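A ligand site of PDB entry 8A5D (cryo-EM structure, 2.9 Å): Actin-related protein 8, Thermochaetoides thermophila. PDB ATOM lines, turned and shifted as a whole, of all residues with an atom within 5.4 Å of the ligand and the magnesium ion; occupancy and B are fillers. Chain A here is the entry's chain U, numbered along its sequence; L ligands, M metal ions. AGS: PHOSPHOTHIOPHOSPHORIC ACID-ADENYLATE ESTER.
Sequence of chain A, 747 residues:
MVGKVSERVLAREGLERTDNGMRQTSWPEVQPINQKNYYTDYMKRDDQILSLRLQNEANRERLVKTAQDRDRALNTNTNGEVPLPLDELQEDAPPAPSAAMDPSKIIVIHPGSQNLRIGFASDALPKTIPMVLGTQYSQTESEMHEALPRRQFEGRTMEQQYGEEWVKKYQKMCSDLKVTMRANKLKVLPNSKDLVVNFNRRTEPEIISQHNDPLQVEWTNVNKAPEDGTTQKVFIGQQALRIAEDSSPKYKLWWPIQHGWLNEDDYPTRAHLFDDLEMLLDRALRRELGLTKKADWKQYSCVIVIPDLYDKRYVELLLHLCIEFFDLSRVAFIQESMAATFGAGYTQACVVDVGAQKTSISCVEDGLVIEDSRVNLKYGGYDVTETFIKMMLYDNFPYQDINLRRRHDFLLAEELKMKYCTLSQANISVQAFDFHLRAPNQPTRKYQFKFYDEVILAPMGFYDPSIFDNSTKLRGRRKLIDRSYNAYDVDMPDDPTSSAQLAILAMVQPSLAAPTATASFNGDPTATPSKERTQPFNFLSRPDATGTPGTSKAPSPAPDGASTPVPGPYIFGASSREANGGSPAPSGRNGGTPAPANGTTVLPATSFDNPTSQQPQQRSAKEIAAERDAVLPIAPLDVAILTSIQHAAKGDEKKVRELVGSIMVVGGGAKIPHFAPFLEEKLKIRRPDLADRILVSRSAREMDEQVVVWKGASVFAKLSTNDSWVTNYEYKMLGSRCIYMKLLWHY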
ATOM      1  N   HIS A 110      22.800   7.330  -8.049  1.00  0.00           N
ATOM      2  CA  HIS A 110      21.733   7.645  -9.023  1.00  0.00           C
ATOM      3  C   HIS A 110      21.516   6.414  -9.912  1.00  0.00           C
ATOM      4  O   HIS A 110      22.281   6.266 -10.881  1.00  0.00           O
ATOM      5  CB  HIS A 110      22.057   8.962  -9.755  1.00  0.00           C
ATOM      6  CG  HIS A 110      20.964   9.337 -10.673  1.00  0.00           C
ATOM      7  ND1 HIS A 110      21.079  10.317 -11.596  1.00  0.00           N
ATOM      8  CD2 HIS A 110      19.725   8.832 -10.824  1.00  0.00           C
ATOM      9  CE1 HIS A 110      19.949  10.422 -12.241  1.00  0.00           C
ATOM     10  NE2 HIS A 110      19.125   9.523 -11.826  1.00  0.00           N
ATOM     11  N   PRO A 111      20.633   5.463  -9.510  1.00  0.00           N
ATOM     12  CA  PRO A 111      20.553   4.156 -10.168  1.00  0.00           C
ATOM     13  C   PRO A 111      19.813   4.344 -11.491  1.00  0.00           C
ATOM     14  O   PRO A 111      19.243   5.442 -11.756  1.00  0.00           O
ATOM     15  CB  PRO A 111      19.717   3.280  -9.234  1.00  0.00           C
ATOM     16  CG  PRO A 111      19.831   3.988  -7.900  1.00  0.00           C
ATOM     17  CD  PRO A 111      19.791   5.460  -8.304  1.00  0.00           C
ATOM     18  N   GLY A 112      19.847   3.304 -12.325  1.00  0.00           N
ATOM     19  CA  GLY A 112      19.191   3.432 -13.638  1.00  0.00           C
ATOM     20  C   GLY A 112      19.060   2.116 -14.349  1.00  0.00           C
ATOM     21  O   GLY A 112      19.689   1.114 -13.949  1.00  0.00           O
ATOM     22  N   SER A 113      18.422   2.173 -15.525  1.00  0.00           N
ATOM     23  CA  SER A 113      18.126   0.995 -16.329  1.00  0.00           C
ATOM     24  C   SER A 113      19.269   0.610 -17.285  1.00  0.00           C
ATOM     25  O   SER A 113      19.326  -0.565 -17.661  1.00  0.00           O
ATOM     26  CB  SER A 113      16.816   1.188 -16.975  1.00  0.00           C
ATOM     27  OG  SER A 113      16.764   2.444 -17.544  1.00  0.00           O
ATOM     28  N   GLN A 114      20.125   1.537 -17.708  1.00  0.00           N
ATOM     29  CA  GLN A 114      21.415   1.130 -18.349  1.00  0.00           C
ATOM     30  C   GLN A 114      22.567   1.386 -17.365  1.00  0.00           C
ATOM     31  O   GLN A 114      23.430   0.542 -17.249  1.00  0.00           O
ATOM     32  CB  GLN A 114      21.637   1.800 -19.705  1.00  0.00           C
ATOM     33  CG  GLN A 114      21.278   0.930 -20.891  1.00  0.00           C
ATOM     34  CD  GLN A 114      21.676   1.500 -22.252  1.00  0.00           C
ATOM     35  OE1 GLN A 114      20.835   1.827 -23.094  1.00  0.00           O
ATOM     36  NE2 GLN A 114      22.960   1.571 -22.514  1.00  0.00           N
ATOM     37  N   ASN A 115      22.585   2.513 -16.685  1.00  0.00           N
ATOM     38  CA  ASN A 115      23.792   3.019 -16.008  1.00  0.00           C
ATOM     39  C   ASN A 115      23.514   3.414 -14.550  1.00  0.00           C
ATOM     40  O   ASN A 115      22.577   4.185 -14.294  1.00  0.00           O
ATOM     41  CB  ASN A 115      24.309   4.226 -16.800  1.00  0.00           C
ATOM     42  CG  ASN A 115      24.770   3.873 -18.196  1.00  0.00           C
ATOM     43  OD1 ASN A 115      25.632   2.989 -18.377  1.00  0.00           O
ATOM     44  ND2 ASN A 115      24.211   4.539 -19.186  1.00  0.00           N
ATOM     45  N   ARG A 117      25.300   5.740 -11.555  1.00  0.00           N
ATOM     46  CA  ARG A 117      26.266   6.827 -11.289  1.00  0.00           C
ATOM     47  C   ARG A 117      26.460   6.951  -9.780  1.00  0.00           C
ATOM     48  O   ARG A 117      25.490   7.111  -9.088  1.00  0.00           O
ATOM     49  CB  ARG A 117      25.790   8.120 -11.920  1.00  0.00           C
ATOM     50  CG  ARG A 117      25.580   7.848 -13.383  1.00  0.00           C
ATOM     51  CD  ARG A 117      25.221   8.994 -14.206  1.00  0.00           C
ATOM     52  NE  ARG A 117      25.424   8.541 -15.570  1.00  0.00           N
ATOM     53  CZ  ARG A 117      24.462   8.187 -16.410  1.00  0.00           C
ATOM     54  NH1 ARG A 117      23.218   8.168 -16.014  1.00  0.00           N
ATOM     55  NH2 ARG A 117      24.781   7.835 -17.632  1.00  0.00           N
ATOM     56  N   GLY A 260      12.607   1.851 -16.070  1.00  0.00           N
ATOM     57  CA  GLY A 260      12.708   2.787 -14.945  1.00  0.00           C
ATOM     58  C   GLY A 260      12.001   2.309 -13.721  1.00  0.00           C
ATOM     59  O   GLY A 260      11.684   3.160 -12.874  1.00  0.00           O
ATOM     60  N   GLU A 336      14.628  13.313  -9.334  1.00  0.00           N
ATOM     61  CA  GLU A 336      15.443  13.586 -10.564  1.00  0.00           C
ATOM     62  C   GLU A 336      15.254  15.041 -11.003  1.00  0.00           C
ATOM     63  O   GLU A 336      16.255  15.717 -11.206  1.00  0.00           O
ATOM     64  CB  GLU A 336      15.185  12.643 -11.737  1.00  0.00           C
ATOM     65  CG  GLU A 336      15.723  11.235 -11.468  1.00  0.00           C
ATOM     66  CD  GLU A 336      15.470  10.112 -12.490  1.00  0.00           C
ATOM     67  OE1 GLU A 336      14.436  10.147 -13.193  1.00  0.00           O
ATOM     68  OE2 GLU A 336      16.339   9.202 -12.606  1.00  0.00           O
ATOM     69  N   ASP A 353      13.984  14.604 -19.103  1.00  0.00           N
ATOM     70  CA  ASP A 353      15.096  13.675 -18.784  1.00  0.00           C
ATOM     71  C   ASP A 353      14.894  12.463 -19.670  1.00  0.00           C
ATOM     72  O   ASP A 353      14.003  11.709 -19.368  1.00  0.00           O
ATOM     73  CB  ASP A 353      15.221  13.337 -17.287  1.00  0.00           C
ATOM     74  CG  ASP A 353      16.455  12.507 -16.870  1.00  0.00           C
ATOM     75  OD1 ASP A 353      17.045  11.841 -17.713  1.00  0.00           O
ATOM     76  OD2 ASP A 353      16.807  12.493 -15.660  1.00  0.00           O
ATOM     77  N   VAL A 354      15.747  12.306 -20.669  1.00  0.00           N
ATOM     78  CA  VAL A 354      15.590  11.279 -21.726  1.00  0.00           C
ATOM     79  C   VAL A 354      16.662  10.243 -21.430  1.00  0.00           C
ATOM     80  O   VAL A 354      17.836  10.537 -21.540  1.00  0.00           O
ATOM     81  CB  VAL A 354      15.740  11.863 -23.148  1.00  0.00           C
ATOM     82  CG1 VAL A 354      15.295  10.845 -24.184  1.00  0.00           C
ATOM     83  CG2 VAL A 354      14.974  13.145 -23.319  1.00  0.00           C
ATOM     84  N   GLY A 355      16.280   9.017 -21.248  1.00  0.00           N
ATOM     85  CA  GLY A 355      17.234   8.035 -20.734  1.00  0.00           C
ATOM     86  C   GLY A 355      17.304   6.883 -21.625  1.00  0.00           C
ATOM     87  O   GLY A 355      16.911   7.082 -22.744  1.00  0.00           O
ATOM     88  N   ALA A 356      17.812   5.756 -21.154  1.00  0.00           N
ATOM     89  CA  ALA A 356      17.842   4.505 -21.937  1.00  0.00           C
ATOM     90  C   ALA A 356      16.422   4.047 -22.117  1.00  0.00           C
ATOM     91  O   ALA A 356      16.022   3.821 -23.307  1.00  0.00           O
ATOM     92  CB  ALA A 356      18.636   3.460 -21.256  1.00  0.00           C
ATOM     93  N   GLN A 357      15.657   3.968 -21.015  1.00  0.00           N
ATOM     94  CA  GLN A 357      14.379   3.229 -21.046  1.00  0.00           C
ATOM     95  C   GLN A 357      13.165   3.994 -20.546  1.00  0.00           C
ATOM     96  O   GLN A 357      12.025   3.446 -20.662  1.00  0.00           O
ATOM     97  CB  GLN A 357      14.565   1.897 -20.377  1.00  0.00           C
ATOM     98  CG  GLN A 357      15.610   1.041 -21.043  1.00  0.00           C
ATOM     99  CD  GLN A 357      15.448  -0.360 -20.576  1.00  0.00           C
ATOM    100  OE1 GLN A 357      15.099  -0.534 -19.438  1.00  0.00           O
ATOM    101  NE2 GLN A 357      15.717  -1.360 -21.406  1.00  0.00           N
ATOM    102  N   LYS A 358      13.343   5.242 -20.282  1.00  0.00           N
ATOM    103  CA  LYS A 358      12.278   6.075 -19.705  1.00  0.00           C
ATOM    104  C   LYS A 358      12.578   7.487 -20.157  1.00  0.00           C
ATOM    105  O   LYS A 358      13.739   7.927 -20.210  1.00  0.00           O
ATOM    106  CB  LYS A 358      12.373   5.920 -18.170  1.00  0.00           C
ATOM    107  CG  LYS A 358      11.694   6.986 -17.384  1.00  0.00           C
ATOM    108  CD  LYS A 358      11.978   6.878 -15.912  1.00  0.00           C
ATOM    109  CE  LYS A 358      13.350   7.396 -15.547  1.00  0.00           C
ATOM    110  NZ  LYS A 358      13.551   8.875 -15.684  1.00  0.00           N
ATOM    111  N   GLY A 381      16.468   6.120 -25.300  1.00  0.00           N
ATOM    112  CA  GLY A 381      17.535   5.912 -26.278  1.00  0.00           C
ATOM    113  C   GLY A 381      17.721   4.461 -26.605  1.00  0.00           C
ATOM    114  O   GLY A 381      18.274   4.240 -27.708  1.00  0.00           O
ATOM    115  N   TYR A 382      17.249   3.523 -25.789  1.00  0.00           N
ATOM    116  CA  TYR A 382      17.382   2.081 -26.140  1.00  0.00           C
ATOM    117  C   TYR A 382      16.441   1.721 -27.276  1.00  0.00           C
ATOM    118  O   TYR A 382      16.840   0.954 -28.205  1.00  0.00           O
ATOM    119  CB  TYR A 382      17.138   1.167 -24.952  1.00  0.00           C
ATOM    120  CG  TYR A 382      17.329  -0.278 -25.310  1.00  0.00           C
ATOM    121  CD1 TYR A 382      18.566  -0.758 -25.709  1.00  0.00           C
ATOM    122  CD2 TYR A 382      16.278  -1.180 -25.247  1.00  0.00           C
ATOM    123  CE1 TYR A 382      18.738  -2.092 -26.036  1.00  0.00           C
ATOM    124  CE2 TYR A 382      16.441  -2.511 -25.542  1.00  0.00           C
ATOM    125  CZ  TYR A 382      17.682  -2.976 -25.958  1.00  0.00           C
ATOM    126  OH  TYR A 382      17.882  -4.297 -26.278  1.00  0.00           O
ATOM    127  N   THR A 385      18.162   2.676 -30.451  1.00  0.00           N
ATOM    128  CA  THR A 385      19.127   1.608 -30.857  1.00  0.00           C
ATOM    129  C   THR A 385      18.362   0.486 -31.574  1.00  0.00           C
ATOM    130  O   THR A 385      18.752   0.147 -32.661  1.00  0.00           O
ATOM    131  CB  THR A 385      19.910   1.102 -29.637  1.00  0.00           C
ATOM    132  OG1 THR A 385      20.620   2.182 -29.021  1.00  0.00           O
ATOM    133  CG2 THR A 385      20.878  -0.007 -29.961  1.00  0.00           C
ATOM    134  N   GLU A 414      24.933  -0.271 -29.614  1.00  0.00           N
ATOM    135  CA  GLU A 414      25.134   1.001 -28.884  1.00  0.00           C
ATOM    136  C   GLU A 414      26.206   1.862 -29.585  1.00  0.00           C
ATOM    137  O   GLU A 414      25.956   3.072 -29.789  1.00  0.00           O
ATOM    138  CB  GLU A 414      25.459   0.722 -27.416  1.00  0.00           C
ATOM    139  CG  GLU A 414      24.240   0.282 -26.604  1.00  0.00           C
ATOM    140  CD  GLU A 414      23.209   1.373 -26.307  1.00  0.00           C
ATOM    141  OE1 GLU A 414      23.414   2.188 -25.372  1.00  0.00           O
ATOM    142  OE2 GLU A 414      22.188   1.417 -27.035  1.00  0.00           O
ATOM    143  N   LYS A 417      24.940   3.283 -32.940  1.00  0.00           N
ATOM    144  CA  LYS A 417      23.909   4.312 -32.699  1.00  0.00           C
ATOM    145  C   LYS A 417      24.601   5.625 -32.269  1.00  0.00           C
ATOM    146  O   LYS A 417      24.187   6.703 -32.791  1.00  0.00           O
ATOM    147  CB  LYS A 417      22.869   3.821 -31.696  1.00  0.00           C
ATOM    148  CG  LYS A 417      21.601   4.678 -31.638  1.00  0.00           C
ATOM    149  CD  LYS A 417      21.628   5.775 -30.587  1.00  0.00           C
ATOM    150  CE  LYS A 417      21.443   5.188 -29.206  1.00  0.00           C
ATOM    151  NZ  LYS A 417      21.330   6.236 -28.162  1.00  0.00           N
ATOM    152  N   MET A 418      25.608   5.560 -31.390  1.00  0.00           N
ATOM    153  CA  MET A 418      26.335   6.764 -30.922  1.00  0.00           C
ATOM    154  C   MET A 418      27.107   7.446 -32.052  1.00  0.00           C
ATOM    155  O   MET A 418      27.161   8.689 -32.042  1.00  0.00           O
ATOM    156  CB  MET A 418      27.289   6.443 -29.773  1.00  0.00           C
ATOM    157  CG  MET A 418      26.548   6.122 -28.487  1.00  0.00           C
ATOM    158  SD  MET A 418      27.651   5.928 -27.052  1.00  0.00           S
ATOM    159  CE  MET A 418      26.564   5.021 -25.951  1.00  0.00           C
ATOM    160  N   GLY A 667      19.966  13.787 -19.430  1.00  0.00           N
ATOM    161  CA  GLY A 667      19.974  12.334 -19.624  1.00  0.00           C
ATOM    162  C   GLY A 667      20.714  11.942 -20.893  1.00  0.00           C
ATOM    163  O   GLY A 667      20.811  12.737 -21.856  1.00  0.00           O
ATOM    164  N   GLY A 668      21.204  10.719 -20.925  1.00  0.00           N
ATOM    165  CA  GLY A 668      21.971  10.253 -22.088  1.00  0.00           C
ATOM    166  C   GLY A 668      21.175  10.140 -23.394  1.00  0.00           C
ATOM    167  O   GLY A 668      21.783  10.255 -24.420  1.00  0.00           O
ATOM    168  N   GLY A 669      19.890   9.867 -23.380  1.00  0.00           N
ATOM    169  CA  GLY A 669      19.092   9.713 -24.618  1.00  0.00           C
ATOM    170  C   GLY A 669      19.012  11.015 -25.350  1.00  0.00           C
ATOM    171  O   GLY A 669      18.816  10.955 -26.590  1.00  0.00           O
ATOM    172  N   LYS A 671      21.411  12.965 -25.884  1.00  0.00           N
ATOM    173  CA  LYS A 671      22.810  13.296 -26.242  1.00  0.00           C
ATOM    174  C   LYS A 671      23.013  13.057 -27.730  1.00  0.00           C
ATOM    175  O   LYS A 671      24.144  13.374 -28.195  1.00  0.00           O
ATOM    176  CB  LYS A 671      23.747  12.504 -25.329  1.00  0.00           C
ATOM    177  CG  LYS A 671      25.067  13.148 -25.028  1.00  0.00           C
ATOM    178  CD  LYS A 671      25.780  12.480 -23.901  1.00  0.00           C
ATOM    179  CE  LYS A 671      27.256  12.811 -23.856  1.00  0.00           C
ATOM    180  NZ  LYS A 671      27.959  12.225 -22.693  1.00  0.00           N
ATOM    181  N   ILE A 672      21.972  12.630 -28.460  1.00  0.00           N
ATOM    182  CA  ILE A 672      21.835  12.681 -29.959  1.00  0.00           C
ATOM    183  C   ILE A 672      22.100  14.103 -30.461  1.00  0.00           C
ATOM    184  O   ILE A 672      21.673  15.088 -29.846  1.00  0.00           O
ATOM    185  CB  ILE A 672      20.434  12.208 -30.370  1.00  0.00           C
ATOM    186  CG1 ILE A 672      20.297  10.686 -30.262  1.00  0.00           C
ATOM    187  CG2 ILE A 672      20.073  12.675 -31.753  1.00  0.00           C
ATOM    188  CD1 ILE A 672      18.866  10.199 -30.328  1.00  0.00           C
ATOM    189  N   PRO A 673      22.905  14.268 -31.546  1.00  0.00           N
ATOM    190  CA  PRO A 673      23.142  15.584 -32.147  1.00  0.00           C
ATOM    191  C   PRO A 673      21.890  16.330 -32.614  1.00  0.00           C
ATOM    192  O   PRO A 673      20.973  15.689 -33.156  1.00  0.00           O
ATOM    193  CB  PRO A 673      23.996  15.256 -33.359  1.00  0.00           C
ATOM    194  CG  PRO A 673      24.739  14.039 -32.930  1.00  0.00           C
ATOM    195  CD  PRO A 673      23.708  13.229 -32.189  1.00  0.00           C
ATOM    196  N   GLN A 706      24.515  13.643 -19.000  1.00  0.00           N
ATOM    197  CA  GLN A 706      24.440  12.411 -18.181  1.00  0.00           C
ATOM    198  C   GLN A 706      24.769  12.652 -16.704  1.00  0.00           C
ATOM    199  O   GLN A 706      24.461  11.733 -15.916  1.00  0.00           O
ATOM    200  CB  GLN A 706      25.344  11.327 -18.753  1.00  0.00           C
ATOM    201  CG  GLN A 706      24.825  10.795 -20.078  1.00  0.00           C
ATOM    202  CD  GLN A 706      25.741   9.755 -20.698  1.00  0.00           C
ATOM    203  OE1 GLN A 706      26.830  10.095 -21.153  1.00  0.00           O
ATOM    204  NE2 GLN A 706      25.296   8.497 -20.748  1.00  0.00           N
HETATM  205  PG  AGS L   1      17.308   5.794 -17.043  1.00  0.00           P
HETATM  206  S1G AGS L   1      15.865   5.114 -17.866  1.00  0.00           S
HETATM  207  O2G AGS L   1      17.690   5.109 -15.737  1.00  0.00           O
HETATM  208  O3G AGS L   1      17.296   7.323 -16.953  1.00  0.00           O
HETATM  209  PB  AGS L   1      19.908   5.639 -17.703  1.00  0.00           P
HETATM  210  O1B AGS L   1      19.918   6.757 -16.736  1.00  0.00           O
HETATM  211  O2B AGS L   1      20.428   4.291 -17.447  1.00  0.00           O
HETATM  212  O3B AGS L   1      18.383   5.476 -18.115  1.00  0.00           O
HETATM  213  PA  AGS L   1      21.263   7.310 -19.351  1.00  0.00           P
HETATM  214  O1A AGS L   1      22.585   6.821 -18.851  1.00  0.00           O
HETATM  215  O2A AGS L   1      20.679   8.616 -18.926  1.00  0.00           O
HETATM  216  O3A AGS L   1      20.288   6.137 -19.123  1.00  0.00           O
HETATM  217  O5' AGS L   1      21.259   7.258 -20.961  1.00  0.00           O
HETATM  218  C5' AGS L   1      21.804   6.121 -21.593  1.00  0.00           C
HETATM  219  C4' AGS L   1      21.463   6.212 -23.064  1.00  0.00           C
HETATM  220  O4' AGS L   1      22.240   7.302 -23.612  1.00  0.00           O
HETATM  221  C3' AGS L   1      21.865   4.961 -23.869  1.00  0.00           C
HETATM  222  O3' AGS L   1      20.718   4.450 -24.517  1.00  0.00           O
HETATM  223  C2' AGS L   1      22.953   5.461 -24.832  1.00  0.00           C
HETATM  224  O2' AGS L   1      22.914   4.806 -26.085  1.00  0.00           O
HETATM  225  C1' AGS L   1      22.676   6.972 -24.908  1.00  0.00           C
HETATM  226  N9  AGS L   1      23.843   7.777 -25.216  1.00  0.00           N
HETATM  227  C8  AGS L   1      24.947   8.027 -24.424  1.00  0.00           C
HETATM  228  N7  AGS L   1      25.880   8.750 -24.998  1.00  0.00           N
HETATM  229  C5  AGS L   1      25.352   8.994 -26.252  1.00  0.00           C
HETATM  230  C6  AGS L   1      25.876   9.693 -27.350  1.00  0.00           C
HETATM  231  N6  AGS L   1      27.068  10.265 -27.328  1.00  0.00           N
HETATM  232  N1  AGS L   1      25.120   9.764 -28.474  1.00  0.00           N
HETATM  233  C2  AGS L   1      23.924   9.165 -28.472  1.00  0.00           C
HETATM  234  N3  AGS L   1      23.336   8.458 -27.504  1.00  0.00           N
HETATM  235  C4  AGS L   1      24.113   8.411 -26.407  1.00  0.00           C
HETATM  236 MG    MG M   1      18.462   8.484 -15.805  1.00  0.00          MG
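The guanidinium group (NH2) of Arg 117 lies within salt-bridge range of an oxygen (O1A) of the ligand (2.7 Å).
The side-chain carboxylate (OE1) of Glu 414 sits at hydrogen-bond distance from an oxygen (O2') of the ligand, 2.8 Å away.
The backbone NH (N) of Gln 114 lies within hydrogen-bond range of an oxygen (O2B) of the ligand, 2.8 Å away.
O3' of the ligand is in hydrogen-bond range of OE1 of Gln 114.
N of Asn 115 is in hydrogen-bond range of O2B of the ligand (2.9 Å).
The side-chain amide nitrogen (ND2) of Asn 115 lies within hydrogen-bond range of an oxygen (O1A) of the ligand, at 2.8 Å.
O2G of the ligand is in hydrogen-bond range of N of Ser 113 (3.0 Å).
The side-chain hydroxyl (OG) of Ser 113 lies close to a sulfur (S1G) of the ligand, at 2.8 Å.
The backbone NH (N) of Gly 668 sits at hydrogen-bond distance from an oxygen (O2A) of the ligand (2.9 Å).
An oxygen (O2') of the ligand is in hydrogen-bond range of the side-chain amino group (NZ) of Lys 417, at 3.0 Å.
An oxygen (O3B) of the ligand lies within hydrogen-bond range of the backbone NH (N) of Ala 356 (3.1 Å).
N of Gln 357 lies close to S1G of the ligand, 3.4 Å away.
An oxygen (O4') of the ligand sits at hydrogen-bond distance from the backbone NH of Gly 669 (3.5 Å).
S1G of the ligand lies close to N of Lys 358 (3.5 Å).
The side-chain amide nitrogen (NE2) of Gln 706 lies close to the guanidinium group (NH2) of Arg 117 (3.2 Å).
NE2 of Gln 114 lies within hydrogen-bond range of OE1 of Glu 414 (3.0 Å).
OE2 of Glu 414 sits at hydrogen-bond distance from OG1 of Thr 385.
The backbone carbonyl oxygen (O) of Ala 356 is in hydrogen-bond range of the backbone NH (N) of Gly 381 (3.1 Å).
O of Ala 356 lies within hydrogen-bond range of N of Tyr 382 (2.8 Å).
The backbone carbonyl oxygen (O) of Gly 355 sits at hydrogen-bond distance from the backbone NH (N) of Gly 381, at 2.8 Å.
The side-chain amide oxygen (OE1) of Gln 706 is in hydrogen-bond range of the side-chain amino group (NZ) of Lys 671 (2.9 Å).
The side-chain carboxylate of Glu 336 sits at hydrogen-bond distance from a ring nitrogen (NE2) of His 110, at 2.9 Å.
Merely in contact with the ligand: Gly 112 (3.1 Å), Gly 381 (3.7 Å), Met 418 (3.7 Å), Gln 706 (3.7 Å), Lys 671 (3.8 Å), Tyr 382 (3.8 Å), Gly 355 (3.8 Å), Gly 667 (3.8 Å) and Ile 672 (3.98 Å).
Of the 28 residues printed, 20 come within 4 Å of the ligand.
Glu 336 touches the magnesium ion.
Of the 28 residues printed, 1 comes within 4 Å of the magnesium ion.
The magnesium ion is bound by O3G of the ligand (2.0 Å) and O1B of the ligand (2.4 Å).
The magnesium ion has two donor atoms within binding distance.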
